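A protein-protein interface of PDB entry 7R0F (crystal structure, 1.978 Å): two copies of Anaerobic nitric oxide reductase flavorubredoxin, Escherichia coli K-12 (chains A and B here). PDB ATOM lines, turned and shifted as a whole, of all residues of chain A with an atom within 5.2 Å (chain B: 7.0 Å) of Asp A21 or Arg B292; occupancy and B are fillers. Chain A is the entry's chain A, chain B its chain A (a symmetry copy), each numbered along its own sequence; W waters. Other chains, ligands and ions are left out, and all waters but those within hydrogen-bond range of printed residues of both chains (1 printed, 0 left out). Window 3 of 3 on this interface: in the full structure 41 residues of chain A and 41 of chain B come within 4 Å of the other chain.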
ATOM      1  N   VAL A  19       4.079 -12.331  26.061  1.00  0.00           N
ATOM      2  CA  VAL A  19       3.241 -11.832  24.971  1.00  0.00           C
ATOM      3  C   VAL A  19       3.096 -12.854  23.840  1.00  0.00           C
ATOM      4  O   VAL A  19       4.070 -13.479  23.412  1.00  0.00           O
ATOM      5  CB  VAL A  19       3.780 -10.492  24.404  1.00  0.00           C
ATOM      6  CG1 VAL A  19       5.180 -10.656  23.815  1.00  0.00           C
ATOM      7  CG2 VAL A  19       2.817  -9.922  23.371  1.00  0.00           C
ATOM      8  N   ARG A  20       1.862 -13.035  23.382  1.00  0.00           N
ATOM      9  CA  ARG A  20       1.561 -14.005  22.338  1.00  0.00           C
ATOM     10  C   ARG A  20       0.735 -13.381  21.217  1.00  0.00           C
ATOM     11  O   ARG A  20       0.575 -13.975  20.153  1.00  0.00           O
ATOM     12  CB  ARG A  20       0.823 -15.211  22.926  1.00  0.00           C
ATOM     13  CG  ARG A  20       1.696 -16.129  23.772  1.00  0.00           C
ATOM     14  CD  ARG A  20       2.740 -16.836  22.923  1.00  0.00           C
ATOM     15  NE  ARG A  20       3.614 -17.697  23.716  1.00  0.00           N
ATOM     16  CZ  ARG A  20       4.779 -17.313  24.229  1.00  0.00           C
ATOM     17  NH1 ARG A  20       5.219 -16.077  24.034  1.00  0.00           N
ATOM     18  NH2 ARG A  20       5.509 -18.165  24.937  1.00  0.00           N
ATOM     19  N   ASP A  21       0.213 -12.182  21.460  1.00  0.00           N
ATOM     20  CA  ASP A  21      -0.661 -11.522  20.493  1.00  0.00           C
ATOM     21  C   ASP A  21      -0.242 -10.085  20.185  1.00  0.00           C
ATOM     22  O   ASP A  21      -0.138  -9.249  21.083  1.00  0.00           O
ATOM     23  CB  ASP A  21      -2.107 -11.536  20.995  1.00  0.00           C
ATOM     24  CG  ASP A  21      -2.798 -12.862  20.745  1.00  0.00           C
ATOM     25  OD1 ASP A  21      -2.697 -13.384  19.615  1.00  0.00           O
ATOM     26  OD2 ASP A  21      -3.444 -13.384  21.679  1.00  0.00           O
ATOM     27  N   PHE A  22      -0.003  -9.810  18.906  1.00  0.00           N
ATOM     28  CA  PHE A  22       0.280  -8.457  18.437  1.00  0.00           C
ATOM     29  C   PHE A  22      -0.744  -8.038  17.389  1.00  0.00           C
ATOM     30  O   PHE A  22      -1.285  -8.884  16.677  1.00  0.00           O
ATOM     31  CB  PHE A  22       1.695  -8.366  17.862  1.00  0.00           C
ATOM     32  CG  PHE A  22       2.696  -7.765  18.808  1.00  0.00           C
ATOM     33  CD1 PHE A  22       3.240  -8.518  19.835  1.00  0.00           C
ATOM     34  CD2 PHE A  22       3.093  -6.445  18.669  1.00  0.00           C
ATOM     35  CE1 PHE A  22       4.160  -7.965  20.706  1.00  0.00           C
ATOM     36  CE2 PHE A  22       4.014  -5.888  19.536  1.00  0.00           C
ATOM     37  CZ  PHE A  22       4.547  -6.650  20.556  1.00  0.00           C
ATOM     38  N   HIS A  23      -1.002  -6.734  17.303  1.00  0.00           N
ATOM     39  CA  HIS A  23      -1.986  -6.186  16.370  1.00  0.00           C
ATOM     40  C   HIS A  23      -3.331  -6.886  16.528  1.00  0.00           C
ATOM     41  O   HIS A  23      -3.896  -7.393  15.559  1.00  0.00           O
ATOM     42  CB  HIS A  23      -1.491  -6.310  14.927  1.00  0.00           C
ATOM     43  CG  HIS A  23      -0.185  -5.623  14.673  1.00  0.00           C
ATOM     44  ND1 HIS A  23       0.727  -6.079  13.746  1.00  0.00           N
ATOM     45  CD2 HIS A  23       0.361  -4.516  15.228  1.00  0.00           C
ATOM     46  CE1 HIS A  23       1.780  -5.280  13.740  1.00  0.00           C
ATOM     47  NE2 HIS A  23       1.583  -4.324  14.629  1.00  0.00           N
ATOM     48  N   GLY A  24      -3.832  -6.918  17.759  1.00  0.00           N
ATOM     49  CA  GLY A  24      -5.006  -7.706  18.079  1.00  0.00           C
ATOM     50  C   GLY A  24      -4.591  -9.152  18.263  1.00  0.00           C
ATOM     51  O   GLY A  24      -3.884  -9.486  19.211  1.00  0.00           O
ATOM     52  N   THR A  25      -5.033 -10.013  17.352  1.00  0.00           N
ATOM     53  CA  THR A  25      -4.585 -11.400  17.331  1.00  0.00           C
ATOM     54  C   THR A  25      -4.046 -11.748  15.949  1.00  0.00           C
ATOM     55  O   THR A  25      -4.012 -12.916  15.559  1.00  0.00           O
ATOM     56  CB  THR A  25      -5.718 -12.378  17.700  1.00  0.00           C
ATOM     57  OG1 THR A  25      -6.757 -12.305  16.716  1.00  0.00           O
ATOM     58  CG2 THR A  25      -6.291 -12.042  19.069  1.00  0.00           C
ATOM     59  N   TYR A  27      -0.946 -11.100  14.710  1.00  0.00           N
ATOM     60  CA  TYR A  27       0.426 -11.584  14.710  1.00  0.00           C
ATOM     61  C   TYR A  27       0.723 -12.353  15.990  1.00  0.00           C
ATOM     62  O   TYR A  27       0.824 -11.767  17.068  1.00  0.00           O
ATOM     63  CB  TYR A  27       1.420 -10.433  14.546  1.00  0.00           C
ATOM     64  CG  TYR A  27       2.826 -10.896  14.220  1.00  0.00           C
ATOM     65  CD1 TYR A  27       3.684 -11.338  15.219  1.00  0.00           C
ATOM     66  CD2 TYR A  27       3.291 -10.894  12.911  1.00  0.00           C
ATOM     67  CE1 TYR A  27       4.965 -11.765  14.924  1.00  0.00           C
ATOM     68  CE2 TYR A  27       4.571 -11.319  12.607  1.00  0.00           C
ATOM     69  CZ  TYR A  27       5.404 -11.752  13.618  1.00  0.00           C
ATOM     70  OH  TYR A  27       6.680 -12.175  13.322  1.00  0.00           O
ATOM     71  N   LYS A  28       0.860 -13.667  15.858  1.00  0.00           N
ATOM     72  CA  LYS A  28       1.198 -14.519  16.991  1.00  0.00           C
ATOM     73  C   LYS A  28       2.697 -14.487  17.263  1.00  0.00           C
ATOM     74  O   LYS A  28       3.499 -14.866  16.409  1.00  0.00           O
ATOM     75  CB  LYS A  28       0.744 -15.959  16.735  1.00  0.00           C
ATOM     76  CG  LYS A  28      -0.756 -16.125  16.530  1.00  0.00           C
ATOM     77  CD  LYS A  28      -1.527 -15.897  17.818  1.00  0.00           C
ATOM     78  CE  LYS A  28      -3.004 -16.208  17.636  1.00  0.00           C
ATOM     79  NZ  LYS A  28      -3.761 -16.095  18.916  1.00  0.00           N
ATOM     80  N   THR A  29       3.076 -14.020  18.448  1.00  0.00           N
ATOM     81  CA  THR A  29       4.475 -14.031  18.857  1.00  0.00           C
ATOM     82  C   THR A  29       4.749 -15.257  19.721  1.00  0.00           C
ATOM     83  O   THR A  29       4.637 -15.203  20.945  1.00  0.00           O
ATOM     84  CB  THR A  29       4.855 -12.755  19.631  1.00  0.00           C
ATOM     85  OG1 THR A  29       3.972 -12.587  20.747  1.00  0.00           O
ATOM     86  CG2 THR A  29       4.761 -11.537  18.726  1.00  0.00           C
ATOM     87  N   TYR B 258     -16.893  -6.168  16.290  1.00  0.00           N
ATOM     88  CA  TYR B 258     -15.748  -5.492  15.705  1.00  0.00           C
ATOM     89  C   TYR B 258     -14.474  -6.297  15.908  1.00  0.00           C
ATOM     90  O   TYR B 258     -14.447  -7.245  16.692  1.00  0.00           O
ATOM     91  CB  TYR B 258     -15.583  -4.104  16.332  1.00  0.00           C
ATOM     92  CG  TYR B 258     -15.377  -4.165  17.828  1.00  0.00           C
ATOM     93  CD1 TYR B 258     -16.462  -4.174  18.697  1.00  0.00           C
ATOM     94  CD2 TYR B 258     -14.102  -4.236  18.374  1.00  0.00           C
ATOM     95  CE1 TYR B 258     -16.282  -4.245  20.062  1.00  0.00           C
ATOM     96  CE2 TYR B 258     -13.913  -4.308  19.740  1.00  0.00           C
ATOM     97  CZ  TYR B 258     -15.007  -4.310  20.579  1.00  0.00           C
ATOM     98  OH  TYR B 258     -14.828  -4.380  21.941  1.00  0.00           O
ATOM     99  N   ASP B 259     -13.417  -5.906  15.207  1.00  0.00           N
ATOM    100  CA  ASP B 259     -12.078  -6.365  15.543  1.00  0.00           C
ATOM    101  C   ASP B 259     -11.179  -5.143  15.677  1.00  0.00           C
ATOM    102  O   ASP B 259     -11.397  -4.128  15.014  1.00  0.00           O
ATOM    103  CB  ASP B 259     -11.532  -7.333  14.492  1.00  0.00           C
ATOM    104  CG  ASP B 259     -10.507  -8.299  15.068  1.00  0.00           C
ATOM    105  OD1 ASP B 259      -9.964  -8.016  16.157  1.00  0.00           O
ATOM    106  OD2 ASP B 259     -10.252  -9.346  14.437  1.00  0.00           O
ATOM    107  N   PHE B 288     -19.544  -7.402  20.964  1.00  0.00           N
ATOM    108  CA  PHE B 288     -18.616  -8.521  20.841  1.00  0.00           C
ATOM    109  C   PHE B 288     -17.329  -8.128  20.123  1.00  0.00           C
ATOM    110  O   PHE B 288     -17.359  -7.445  19.104  1.00  0.00           O
ATOM    111  CB  PHE B 288     -19.265  -9.688  20.087  1.00  0.00           C
ATOM    112  CG  PHE B 288     -20.530 -10.197  20.715  1.00  0.00           C
ATOM    113  CD1 PHE B 288     -20.484 -11.092  21.771  1.00  0.00           C
ATOM    114  CD2 PHE B 288     -21.767  -9.799  20.235  1.00  0.00           C
ATOM    115  CE1 PHE B 288     -21.646 -11.567  22.349  1.00  0.00           C
ATOM    116  CE2 PHE B 288     -22.934 -10.272  20.806  1.00  0.00           C
ATOM    117  CZ  PHE B 288     -22.873 -11.158  21.863  1.00  0.00           C
ATOM    118  N   ASN B 289     -16.198  -8.563  20.666  1.00  0.00           N
ATOM    119  CA  ASN B 289     -14.941  -8.540  19.932  1.00  0.00           C
ATOM    120  C   ASN B 289     -14.806  -9.882  19.221  1.00  0.00           C
ATOM    121  O   ASN B 289     -14.697 -10.922  19.872  1.00  0.00           O
ATOM    122  CB  ASN B 289     -13.760  -8.277  20.874  1.00  0.00           C
ATOM    123  CG  ASN B 289     -12.432  -8.135  20.141  1.00  0.00           C
ATOM    124  OD1 ASN B 289     -12.119  -8.901  19.230  1.00  0.00           O
ATOM    125  ND2 ASN B 289     -11.641  -7.148  20.547  1.00  0.00           N
ATOM    126  N   VAL B 290     -14.824  -9.862  17.891  1.00  0.00           N
ATOM    127  CA  VAL B 290     -14.899 -11.094  17.109  1.00  0.00           C
ATOM    128  C   VAL B 290     -13.683 -11.995  17.310  1.00  0.00           C
ATOM    129  O   VAL B 290     -13.762 -13.207  17.116  1.00  0.00           O
ATOM    130  CB  VAL B 290     -15.056 -10.800  15.600  1.00  0.00           C
ATOM    131  CG1 VAL B 290     -16.364 -10.076  15.339  1.00  0.00           C
ATOM    132  CG2 VAL B 290     -13.884  -9.983  15.082  1.00  0.00           C
ATOM    133  N   ALA B 291     -12.560 -11.403  17.703  1.00  0.00           N
ATOM    134  CA  ALA B 291     -11.341 -12.168  17.937  1.00  0.00           C
ATOM    135  C   ALA B 291     -11.370 -12.877  19.287  1.00  0.00           C
ATOM    136  O   ALA B 291     -10.568 -13.775  19.541  1.00  0.00           O
ATOM    137  CB  ALA B 291     -10.122 -11.261  17.845  1.00  0.00           C
ATOM    138  N   ARG B 292     -12.300 -12.475  20.149  1.00  0.00           N
ATOM    139  CA  ARG B 292     -12.326 -12.964  21.523  1.00  0.00           C
ATOM    140  C   ARG B 292     -13.688 -13.533  21.918  1.00  0.00           C
ATOM    141  O   ARG B 292     -13.928 -13.814  23.092  1.00  0.00           O
ATOM    142  CB  ARG B 292     -11.951 -11.837  22.492  1.00  0.00           C
ATOM    143  CG  ARG B 292     -10.688 -11.070  22.127  1.00  0.00           C
ATOM    144  CD  ARG B 292      -9.434 -11.894  22.352  1.00  0.00           C
ATOM    145  NE  ARG B 292      -8.228 -11.082  22.217  1.00  0.00           N
ATOM    146  CZ  ARG B 292      -6.996 -11.530  22.433  1.00  0.00           C
ATOM    147  NH1 ARG B 292      -6.801 -12.791  22.798  1.00  0.00           N
ATOM    148  NH2 ARG B 292      -5.958 -10.718  22.284  1.00  0.00           N
ATOM    149  N   SER B 293     -14.579 -13.699  20.948  1.00  0.00           N
ATOM    150  CA  SER B 293     -15.941 -14.137  21.246  1.00  0.00           C
ATOM    151  C   SER B 293     -16.350 -15.396  20.487  1.00  0.00           C
ATOM    152  O   SER B 293     -15.646 -15.853  19.586  1.00  0.00           O
ATOM    153  CB  SER B 293     -16.934 -13.013  20.943  1.00  0.00           C
ATOM    154  OG  SER B 293     -16.591 -11.826  21.637  1.00  0.00           O
ATOM    155  N   ASP B 294     -17.496 -15.951  20.871  1.00  0.00           N
ATOM    156  CA  ASP B 294     -18.088 -17.084  20.173  1.00  0.00           C
ATOM    157  C   ASP B 294     -18.752 -16.592  18.893  1.00  0.00           C
ATOM    158  O   ASP B 294     -19.669 -15.773  18.937  1.00  0.00           O
ATOM    159  CB  ASP B 294     -19.106 -17.798  21.069  1.00  0.00           C
ATOM    160  CG  ASP B 294     -19.568 -19.131  20.498  1.00  0.00           C
ATOM    161  OD1 ASP B 294     -19.437 -19.353  19.276  1.00  0.00           O
ATOM    162  OD2 ASP B 294     -20.074 -19.961  21.282  1.00  0.00           O
ATOM    163  N   LYS B 322     -10.881 -11.263  10.356  1.00  0.00           N
ATOM    164  CA  LYS B 322     -11.963 -11.932  11.076  1.00  0.00           C
ATOM    165  C   LYS B 322     -13.298 -11.257  10.797  1.00  0.00           C
ATOM    166  O   LYS B 322     -14.346 -11.905  10.810  1.00  0.00           O
ATOM    167  CB  LYS B 322     -11.691 -11.962  12.580  1.00  0.00           C
ATOM    168  CG  LYS B 322     -10.653 -12.986  13.002  1.00  0.00           C
ATOM    169  CD  LYS B 322     -10.569 -13.091  14.515  1.00  0.00           C
ATOM    170  CE  LYS B 322      -9.436 -14.008  14.947  1.00  0.00           C
ATOM    171  NZ  LYS B 322      -8.107 -13.479  14.539  1.00  0.00           N
HETATM  172  O   HOH W   1      -7.422  -9.550  15.605  1.00  0.00           O
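No position is printed for both chains. Of the 5 pairs that touch across the chains among the printed residues, none has its exchanged pair printed and touching as well.
The side-chain carboxylate of Asp A21 lies within salt-bridge range of the guanidinium group of Arg B292 (3.6 Å). The side-chain hydroxyl (OG1) of Thr A25 sits at hydrogen-bond distance from the side-chain amino group (NZ) of Lys B322, at 2.8 Å.
Of chain B, only Arg B292 comes within 4 Å of Asp A21. Arg B292 touches just these residues of chain A: Asp A21, Gly A24 and Thr A25. Of the printed residues of chain A, Lys B322 touches Thr A25. Of the printed residues of chain B, Gly A24 touches Arg B292. Of the printed residues of chain A, Ala B291 touches Thr A25 (3.7 Å). Of the printed residues of chain B, Thr A25 touches Ala B291, Arg B292 and Lys B322. Lys A28 touches none of the printed residues of chain B. Val A19 touches none of the printed residues of chain B. The nearest printed residue of chain B that does not touch Asp A21 is Lys B322 (7.4 Å). The nearest printed residue of chain A that does not touch Lys B322 is Lys A28 (6.6 Å).
The side-chain carboxylate (OD1) of Asp A21 lies within salt-bridge range of the side-chain amino group (NZ) of Lys A28, 3.0 Å away. The backbone NH (N) of Ala B291 lies within hydrogen-bond range of the side-chain amide oxygen (OD1) of Asn B289, 3.0 Å away.
Among the printed residues, pairs that only touch across the chains: Gly A24 with Arg B292 (3.9 Å), Thr A25 with Ala B291 (3.7 Å) and Thr A25 with Arg B292 (3.5 Å).
Water W1 bridges N of Thr A25 and OD1 of Asp B259.
Of the 10 printed residues of chain B, 3 touch a printed residue of chain A. Hydrophobic or aromatic side chains of chain B that line the printed part of chain A: Ala B291. Of the 10 printed residues of chain A, 3 touch a printed residue of chain B.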
